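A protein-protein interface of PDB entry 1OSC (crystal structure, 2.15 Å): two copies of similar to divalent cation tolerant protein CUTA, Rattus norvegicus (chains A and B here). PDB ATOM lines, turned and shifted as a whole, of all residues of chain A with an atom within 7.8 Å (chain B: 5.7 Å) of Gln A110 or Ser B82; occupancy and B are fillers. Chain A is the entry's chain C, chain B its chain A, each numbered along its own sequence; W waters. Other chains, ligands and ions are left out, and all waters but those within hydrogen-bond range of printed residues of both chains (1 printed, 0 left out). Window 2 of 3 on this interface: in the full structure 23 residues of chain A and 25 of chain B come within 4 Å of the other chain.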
ATOM      1  N   TYR A  18      17.770  17.667   0.593  1.00  0.00           N
ATOM      2  CA  TYR A  18      17.288  18.069  -0.793  1.00  0.00           C
ATOM      3  C   TYR A  18      17.027  19.563  -0.991  1.00  0.00           C
ATOM      4  O   TYR A  18      16.048  20.102  -0.424  1.00  0.00           O
ATOM      5  CB  TYR A  18      16.246  17.125  -1.538  1.00  0.00           C
ATOM      6  CG  TYR A  18      16.170  17.472  -3.091  1.00  0.00           C
ATOM      7  CD1 TYR A  18      17.270  17.287  -3.938  1.00  0.00           C
ATOM      8  CD2 TYR A  18      14.991  18.039  -3.677  1.00  0.00           C
ATOM      9  CE1 TYR A  18      17.222  17.711  -5.291  1.00  0.00           C
ATOM     10  CE2 TYR A  18      14.931  18.398  -4.997  1.00  0.00           C
ATOM     11  CZ  TYR A  18      16.039  18.235  -5.841  1.00  0.00           C
ATOM     12  OH  TYR A  18      16.062  18.666  -7.220  1.00  0.00           O
ATOM     13  N   VAL A  19      17.880  20.232  -1.791  1.00  0.00           N
ATOM     14  CA  VAL A  19      17.607  21.557  -2.334  1.00  0.00           C
ATOM     15  C   VAL A  19      16.607  21.526  -3.513  1.00  0.00           C
ATOM     16  O   VAL A  19      16.869  21.010  -4.544  1.00  0.00           O
ATOM     17  CB  VAL A  19      19.002  22.321  -2.642  1.00  0.00           C
ATOM     18  CG1 VAL A  19      18.789  23.788  -3.062  1.00  0.00           C
ATOM     19  CG2 VAL A  19      19.857  22.319  -1.335  1.00  0.00           C
ATOM     20  N   PRO A  20      15.403  22.067  -3.355  1.00  0.00           N
ATOM     21  CA  PRO A  20      14.458  22.056  -4.454  1.00  0.00           C
ATOM     22  C   PRO A  20      15.149  22.743  -5.622  1.00  0.00           C
ATOM     23  O   PRO A  20      15.841  23.747  -5.451  1.00  0.00           O
ATOM     24  CB  PRO A  20      13.350  22.899  -3.901  1.00  0.00           C
ATOM     25  CG  PRO A  20      13.365  22.400  -2.444  1.00  0.00           C
ATOM     26  CD  PRO A  20      14.816  22.610  -2.117  1.00  0.00           C
ATOM     27  N   GLY A  21      14.911  22.133  -6.753  1.00  0.00           N
ATOM     28  CA  GLY A  21      15.308  22.569  -8.085  1.00  0.00           C
ATOM     29  C   GLY A  21      16.786  22.405  -8.328  1.00  0.00           C
ATOM     30  O   GLY A  21      17.186  22.777  -9.391  1.00  0.00           O
ATOM     31  N   VAL A  23      18.291  19.435  -8.814  1.00  0.00           N
ATOM     32  CA  VAL A  23      18.221  18.486  -9.886  1.00  0.00           C
ATOM     33  C   VAL A  23      17.122  18.882 -10.903  1.00  0.00           C
ATOM     34  O   VAL A  23      15.940  19.436 -10.521  1.00  0.00           O
ATOM     35  CB  VAL A  23      18.025  17.037  -9.249  1.00  0.00           C
ATOM     36  CG1 VAL A  23      17.724  15.899 -10.275  1.00  0.00           C
ATOM     37  CG2 VAL A  23      19.471  16.636  -8.540  1.00  0.00           C
ATOM     38  N   PRO A 107      12.576  21.292 -13.507  1.00  0.00           N
ATOM     39  CA  PRO A 107      13.168  21.259 -12.142  1.00  0.00           C
ATOM     40  C   PRO A 107      12.425  20.252 -11.336  1.00  0.00           C
ATOM     41  O   PRO A 107      11.202  20.086 -11.411  1.00  0.00           O
ATOM     42  CB  PRO A 107      12.952  22.718 -11.547  1.00  0.00           C
ATOM     43  CG  PRO A 107      11.655  23.270 -12.328  1.00  0.00           C
ATOM     44  CD  PRO A 107      11.483  22.320 -13.621  1.00  0.00           C
ATOM     45  N   VAL A 108      13.209  19.497 -10.568  1.00  0.00           N
ATOM     46  CA  VAL A 108      12.772  18.427  -9.673  1.00  0.00           C
ATOM     47  C   VAL A 108      12.747  19.138  -8.342  1.00  0.00           C
ATOM     48  O   VAL A 108      13.729  19.777  -7.906  1.00  0.00           O
ATOM     49  CB  VAL A 108      13.757  17.302  -9.624  1.00  0.00           C
ATOM     50  CG1 VAL A 108      13.414  16.457  -8.563  1.00  0.00           C
ATOM     51  CG2 VAL A 108      13.735  16.626 -11.079  1.00  0.00           C
ATOM     52  N   GLU A 109      11.533  19.239  -7.800  1.00  0.00           N
ATOM     53  CA  GLU A 109      11.329  20.019  -6.622  1.00  0.00           C
ATOM     54  C   GLU A 109      11.362  19.121  -5.404  1.00  0.00           C
ATOM     55  O   GLU A 109      11.539  19.669  -4.329  1.00  0.00           O
ATOM     56  CB  GLU A 109       9.835  20.704  -6.666  1.00  0.00           C
ATOM     57  CG  GLU A 109       9.717  21.847  -7.739  1.00  0.00           C
ATOM     58  CD  GLU A 109      10.777  22.874  -7.439  1.00  0.00           C
ATOM     59  OE1 GLU A 109      11.792  23.099  -8.216  1.00  0.00           O
ATOM     60  OE2 GLU A 109      10.669  23.334  -6.298  1.00  0.00           O
ATOM     61  N   GLN A 110      10.945  17.858  -5.538  1.00  0.00           N
ATOM     62  CA  GLN A 110      10.973  16.864  -4.449  1.00  0.00           C
ATOM     63  C   GLN A 110      11.351  15.490  -5.006  1.00  0.00           C
ATOM     64  O   GLN A 110      11.249  15.247  -6.240  1.00  0.00           O
ATOM     65  CB  GLN A 110       9.551  16.679  -3.890  1.00  0.00           C
ATOM     66  CG  GLN A 110       8.863  17.999  -3.271  1.00  0.00           C
ATOM     67  CD  GLN A 110       7.482  17.627  -2.651  1.00  0.00           C
ATOM     68  OE1 GLN A 110       6.423  17.789  -3.266  1.00  0.00           O
ATOM     69  NE2 GLN A 110       7.532  16.993  -1.503  1.00  0.00           N
ATOM     70  N   GLY A 111      11.737  14.543  -4.115  1.00  0.00           N
ATOM     71  CA  GLY A 111      11.604  13.119  -4.461  1.00  0.00           C
ATOM     72  C   GLY A 111      12.340  12.277  -3.447  1.00  0.00           C
ATOM     73  O   GLY A 111      12.343  12.689  -2.274  1.00  0.00           O
ATOM     74  N   ASN A 112      13.008  11.182  -3.845  1.00  0.00           N
ATOM     75  CA  ASN A 112      13.696  10.295  -2.850  1.00  0.00           C
ATOM     76  C   ASN A 112      15.063  10.832  -2.452  1.00  0.00           C
ATOM     77  O   ASN A 112      15.950  10.915  -3.293  1.00  0.00           O
ATOM     78  CB  ASN A 112      13.789   8.847  -3.448  1.00  0.00           C
ATOM     79  CG  ASN A 112      14.217   7.790  -2.367  1.00  0.00           C
ATOM     80  OD1 ASN A 112      14.672   6.674  -2.705  1.00  0.00           O
ATOM     81  ND2 ASN A 112      14.098   8.186  -1.102  1.00  0.00           N
ATOM     82  N   PRO A 113      15.250  11.359  -1.237  1.00  0.00           N
ATOM     83  CA  PRO A 113      16.497  12.076  -0.979  1.00  0.00           C
ATOM     84  C   PRO A 113      17.848  11.308  -1.271  1.00  0.00           C
ATOM     85  O   PRO A 113      18.723  11.941  -1.849  1.00  0.00           O
ATOM     86  CB  PRO A 113      16.361  12.522   0.505  1.00  0.00           C
ATOM     87  CG  PRO A 113      14.754  12.582   0.763  1.00  0.00           C
ATOM     88  CD  PRO A 113      14.318  11.400  -0.066  1.00  0.00           C
ATOM     89  N   TYR A 115      18.267   8.809  -3.465  1.00  0.00           N
ATOM     90  CA  TYR A 115      18.344   8.913  -4.892  1.00  0.00           C
ATOM     91  C   TYR A 115      18.918  10.241  -5.467  1.00  0.00           C
ATOM     92  O   TYR A 115      19.887  10.269  -6.270  1.00  0.00           O
ATOM     93  CB  TYR A 115      17.014   8.619  -5.491  1.00  0.00           C
ATOM     94  CG  TYR A 115      17.118   8.761  -6.977  1.00  0.00           C
ATOM     95  CD1 TYR A 115      17.752   7.763  -7.727  1.00  0.00           C
ATOM     96  CD2 TYR A 115      16.613   9.921  -7.667  1.00  0.00           C
ATOM     97  CE1 TYR A 115      17.821   7.831  -9.115  1.00  0.00           C
ATOM     98  CE2 TYR A 115      16.735   9.989  -9.081  1.00  0.00           C
ATOM     99  CZ  TYR A 115      17.347   8.943  -9.777  1.00  0.00           C
ATOM    100  OH  TYR A 115      17.487   8.958 -11.157  1.00  0.00           O
ATOM    101  N   LEU A 116      18.344  11.344  -4.968  1.00  0.00           N
ATOM    102  CA  LEU A 116      18.758  12.675  -5.414  1.00  0.00           C
ATOM    103  C   LEU A 116      20.194  12.975  -4.977  1.00  0.00           C
ATOM    104  O   LEU A 116      20.878  13.755  -5.664  1.00  0.00           O
ATOM    105  CB  LEU A 116      17.866  13.739  -4.785  1.00  0.00           C
ATOM    106  CG  LEU A 116      16.630  14.286  -5.559  1.00  0.00           C
ATOM    107  CD1 LEU A 116      16.543  13.911  -7.099  1.00  0.00           C
ATOM    108  CD2 LEU A 116      15.368  14.146  -4.840  1.00  0.00           C
ATOM    109  N   GLY B  21       1.614  24.553  -8.565  1.00  0.00           N
ATOM    110  CA  GLY B  21       2.611  23.856  -7.751  1.00  0.00           C
ATOM    111  C   GLY B  21       1.867  22.942  -6.839  1.00  0.00           C
ATOM    112  O   GLY B  21       2.502  22.173  -6.103  1.00  0.00           O
ATOM    113  N   SER B  22       0.531  22.987  -6.844  1.00  0.00           N
ATOM    114  CA  SER B  22      -0.108  22.201  -5.752  1.00  0.00           C
ATOM    115  C   SER B  22      -0.392  20.706  -6.128  1.00  0.00           C
ATOM    116  O   SER B  22      -0.664  19.890  -5.220  1.00  0.00           O
ATOM    117  CB  SER B  22      -1.382  22.837  -5.320  1.00  0.00           C
ATOM    118  OG  SER B  22      -2.291  22.703  -6.371  1.00  0.00           O
ATOM    119  N   VAL B  23      -0.216  20.374  -7.442  1.00  0.00           N
ATOM    120  CA  VAL B  23      -0.201  19.003  -7.933  1.00  0.00           C
ATOM    121  C   VAL B  23       1.231  18.853  -8.551  1.00  0.00           C
ATOM    122  O   VAL B  23       1.782  19.858  -9.064  1.00  0.00           O
ATOM    123  CB  VAL B  23      -1.290  18.811  -9.066  1.00  0.00           C
ATOM    124  CG1 VAL B  23      -1.250  17.519  -9.909  1.00  0.00           C
ATOM    125  CG2 VAL B  23      -2.830  18.819  -8.361  1.00  0.00           C
ATOM    126  N   SER B  24       1.770  17.655  -8.412  1.00  0.00           N
ATOM    127  CA  SER B  24       3.113  17.279  -8.978  1.00  0.00           C
ATOM    128  C   SER B  24       2.904  16.086  -9.839  1.00  0.00           C
ATOM    129  O   SER B  24       1.976  15.259  -9.674  1.00  0.00           O
ATOM    130  CB  SER B  24       4.070  16.953  -7.877  1.00  0.00           C
ATOM    131  OG  SER B  24       4.310  18.127  -7.228  1.00  0.00           O
ATOM    132  N   THR B  80      -0.302  13.437  -8.392  1.00  0.00           N
ATOM    133  CA  THR B  80      -0.921  13.484  -7.123  1.00  0.00           C
ATOM    134  C   THR B  80      -0.648  14.888  -6.518  1.00  0.00           C
ATOM    135  O   THR B  80       0.083  15.772  -7.105  1.00  0.00           O
ATOM    136  CB  THR B  80      -0.245  12.390  -6.314  1.00  0.00           C
ATOM    137  OG1 THR B  80      -0.752  12.394  -4.990  1.00  0.00           O
ATOM    138  CG2 THR B  80       1.369  12.640  -6.103  1.00  0.00           C
ATOM    139  N   GLN B  81      -1.192  15.111  -5.359  1.00  0.00           N
ATOM    140  CA  GLN B  81      -0.986  16.388  -4.695  1.00  0.00           C
ATOM    141  C   GLN B  81       0.434  16.474  -4.270  1.00  0.00           C
ATOM    142  O   GLN B  81       1.005  15.502  -3.800  1.00  0.00           O
ATOM    143  CB  GLN B  81      -1.773  16.439  -3.389  1.00  0.00           C
ATOM    144  CG  GLN B  81      -3.250  16.901  -3.553  1.00  0.00           C
ATOM    145  CD  GLN B  81      -4.016  16.888  -2.169  1.00  0.00           C
ATOM    146  OE1 GLN B  81      -4.772  15.946  -1.864  1.00  0.00           O
ATOM    147  NE2 GLN B  81      -3.798  17.900  -1.381  1.00  0.00           N
ATOM    148  N   SER B  82       0.992  17.685  -4.305  1.00  0.00           N
ATOM    149  CA  SER B  82       2.351  17.859  -3.982  1.00  0.00           C
ATOM    150  C   SER B  82       2.562  17.526  -2.496  1.00  0.00           C
ATOM    151  O   SER B  82       3.590  17.042  -2.139  1.00  0.00           O
ATOM    152  CB  SER B  82       2.805  19.319  -4.202  1.00  0.00           C
ATOM    153  OG  SER B  82       2.743  19.542  -5.545  1.00  0.00           O
ATOM    154  N   SER B  83       1.635  17.947  -1.633  1.00  0.00           N
ATOM    155  CA  SER B  83       1.786  17.753  -0.193  1.00  0.00           C
ATOM    156  C   SER B  83       1.759  16.260   0.171  1.00  0.00           C
ATOM    157  O   SER B  83       2.111  15.914   1.281  1.00  0.00           O
ATOM    158  CB  SER B  83       0.577  18.387   0.556  1.00  0.00           C
ATOM    159  OG  SER B  83      -0.541  17.605   0.108  1.00  0.00           O
ATOM    160  N   LEU B  84       1.283  15.421  -0.728  1.00  0.00           N
ATOM    161  CA  LEU B  84       1.423  14.005  -0.620  1.00  0.00           C
ATOM    162  C   LEU B  84       2.756  13.362  -1.166  1.00  0.00           C
ATOM    163  O   LEU B  84       3.008  12.136  -1.052  1.00  0.00           O
ATOM    164  CB  LEU B  84       0.279  13.429  -1.387  1.00  0.00           C
ATOM    165  CG  LEU B  84      -0.992  12.912  -0.724  1.00  0.00           C
ATOM    166  CD1 LEU B  84      -1.040  13.092   0.802  1.00  0.00           C
ATOM    167  CD2 LEU B  84      -2.252  13.167  -1.487  1.00  0.00           C
ATOM    168  N   VAL B  85       3.587  14.140  -1.838  1.00  0.00           N
ATOM    169  CA  VAL B  85       4.804  13.553  -2.383  1.00  0.00           C
ATOM    170  C   VAL B  85       5.671  12.830  -1.360  1.00  0.00           C
ATOM    171  O   VAL B  85       6.131  11.706  -1.670  1.00  0.00           O
ATOM    172  CB  VAL B  85       5.567  14.425  -3.224  1.00  0.00           C
ATOM    173  CG1 VAL B  85       6.972  13.666  -3.721  1.00  0.00           C
ATOM    174  CG2 VAL B  85       4.724  14.746  -4.539  1.00  0.00           C
ATOM    175  N   PRO B  86       5.825  13.361  -0.146  1.00  0.00           N
ATOM    176  CA  PRO B  86       6.549  12.624   0.916  1.00  0.00           C
ATOM    177  C   PRO B  86       6.017  11.263   1.313  1.00  0.00           C
ATOM    178  O   PRO B  86       6.768  10.286   1.382  1.00  0.00           O
ATOM    179  CB  PRO B  86       6.572  13.626   2.077  1.00  0.00           C
ATOM    180  CG  PRO B  86       6.406  15.051   1.346  1.00  0.00           C
ATOM    181  CD  PRO B  86       5.429  14.717   0.301  1.00  0.00           C
ATOM    182  N   VAL B 103      12.623   8.234  -7.256  1.00  0.00           N
ATOM    183  CA  VAL B 103      11.420   9.061  -7.344  1.00  0.00           C
ATOM    184  C   VAL B 103      11.838  10.505  -7.423  1.00  0.00           C
ATOM    185  O   VAL B 103      12.727  10.886  -6.735  1.00  0.00           O
ATOM    186  CB  VAL B 103      10.280   8.693  -6.282  1.00  0.00           C
ATOM    187  CG1 VAL B 103      10.722   7.686  -5.322  1.00  0.00           C
ATOM    188  CG2 VAL B 103       9.536   9.784  -5.715  1.00  0.00           C
ATOM    189  N   ILE B 104      11.308  11.197  -8.423  1.00  0.00           N
ATOM    190  CA  ILE B 104      11.468  12.590  -8.602  1.00  0.00           C
ATOM    191  C   ILE B 104      10.007  13.126  -8.813  1.00  0.00           C
ATOM    192  O   ILE B 104       9.219  12.498  -9.473  1.00  0.00           O
ATOM    193  CB  ILE B 104      12.262  12.948  -9.771  1.00  0.00           C
ATOM    194  CG1 ILE B 104      11.725  12.417 -11.059  1.00  0.00           C
ATOM    195  CG2 ILE B 104      13.793  12.429  -9.765  1.00  0.00           C
ATOM    196  CD1 ILE B 104      12.630  12.847 -12.142  1.00  0.00           C
ATOM    197  N   ALA B 105       9.722  14.342  -8.360  1.00  0.00           N
ATOM    198  CA  ALA B 105       8.391  14.965  -8.602  1.00  0.00           C
ATOM    199  C   ALA B 105       8.665  16.399  -9.209  1.00  0.00           C
ATOM    200  O   ALA B 105       9.554  17.108  -8.794  1.00  0.00           O
ATOM    201  CB  ALA B 105       7.652  15.085  -7.312  1.00  0.00           C
ATOM    202  N   LEU B 106       7.932  16.704 -10.265  1.00  0.00           N
ATOM    203  CA  LEU B 106       7.986  18.014 -10.898  1.00  0.00           C
ATOM    204  C   LEU B 106       6.661  18.759 -10.751  1.00  0.00           C
ATOM    205  O   LEU B 106       5.663  18.121 -10.930  1.00  0.00           O
ATOM    206  CB  LEU B 106       8.034  17.714 -12.395  1.00  0.00           C
ATOM    207  CG  LEU B 106       9.455  17.025 -12.433  1.00  0.00           C
ATOM    208  CD1 LEU B 106       9.229  15.662 -12.915  1.00  0.00           C
ATOM    209  CD2 LEU B 106      10.415  17.715 -13.270  1.00  0.00           C
ATOM    210  N   PRO B 107       6.711  20.033 -10.446  1.00  0.00           N
ATOM    211  CA  PRO B 107       5.548  20.872 -10.063  1.00  0.00           C
ATOM    212  C   PRO B 107       4.635  21.173 -11.269  1.00  0.00           C
ATOM    213  O   PRO B 107       5.113  21.438 -12.376  1.00  0.00           O
ATOM    214  CB  PRO B 107       6.251  22.178  -9.674  1.00  0.00           C
ATOM    215  CG  PRO B 107       7.457  22.196 -10.629  1.00  0.00           C
ATOM    216  CD  PRO B 107       7.984  20.815 -10.352  1.00  0.00           C
HETATM  217  O   HOH W   1       6.489  19.005  -6.150  1.00  0.00           O
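Among the printed residues, pairs that only touch across the chains: Pro A107 with Leu B106, Pro A107 with Pro B107, Val A108 with Ile B104, Val A108 with Ala B105, Glu A109 with Pro B107, Gln A110 with Val B85, Gln A110 with Pro B86, Gln A110 with Ile B104, Gly A111 with Val B103 and Tyr A115 with Ile B104.
Water W1 bridges the side-chain hydroxyl (OG) of Ser B24 (2.6 Å) and the side-chain amide oxygen (OE1) of Gln A110 (3.1 Å).
Pro A107 touches its own counterpart, Pro B107.
3 positions are printed for both chains.
Printed residues of chain B within 4 Å of Val A108: Ile B104 (3.9 Å) and Ala B105 (3.6 Å).
Of the printed residues of chain B, Glu A109 touches Ala B105 (3.1 Å) and Pro B107 (3.3 Å).
Of the printed residues of chain B, Gln A110 touches Ser B82 (3.1 Å), Val B85 (3.5 Å), Pro B86 (3.6 Å), Ile B104 (3.6 Å) and Ala B105 (2.8 Å).
Printed residues of chain B within 4 Å of Tyr A115: Ile B104 (3.9 Å).
Printed residues of chain A within 4 Å of Ser B82: Gln A110.
Printed residues of chain A within 4 Å of Val B85: Gln A110 (3.5 Å).
The nearest printed residue of chain A that does not touch Val B103 is Tyr A115 (4.1 Å).
OE1 of Gln A110 lies close to O of Ser B82, 3.1 Å away.
O of Val B103 lies within hydrogen-bond range of N of Asn A112 (2.9 Å).
O of Ala B105 lies within hydrogen-bond range of N of Glu A109 (3.1 Å).
The backbone carbonyl oxygen (O) of Gln A110 is in hydrogen-bond range of the backbone NH (N) of Ala B105 (2.8 Å).
The side-chain hydroxyl (OG) of Ser B82 sits at hydrogen-bond distance from the backbone carbonyl oxygen (O) of Gly B21.
The backbone NH (N) of Ser B82 lies within hydrogen-bond range of the backbone carbonyl oxygen (O) of Ser B22, 2.9 Å away.
The side-chain hydroxyl (OG) of Ser B24 is in hydrogen-bond range of the side-chain hydroxyl (OG) of Ser B82 (2.7 Å).
The side-chain hydroxyl (OH) of Tyr A18 is in hydrogen-bond range of the backbone carbonyl oxygen (O) of Val A108.
The backbone NH (N) of Gly A21 is in hydrogen-bond range of the backbone carbonyl oxygen (O) of Val A108, at 2.9 Å.
O of Val A23 is in hydrogen-bond range of N of Val A108.
Of the 16 printed residues of chain B, 8 touch a printed residue of chain A.
Hydrophobic or aromatic side chains of chain B that line the printed part of chain A: Val B85, Pro B86, Val B103, Ile B104, Ala B105, Leu B106 and Pro B107.
Printed residues of chain A that touch a printed residue of chain B: Pro A107, Val A108, Glu A109, Gln A110, Gly A111, Asn A112 and Tyr A115.
Along chain A the printed residues that touch a printed residue of chain B span positions 107 to 115.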
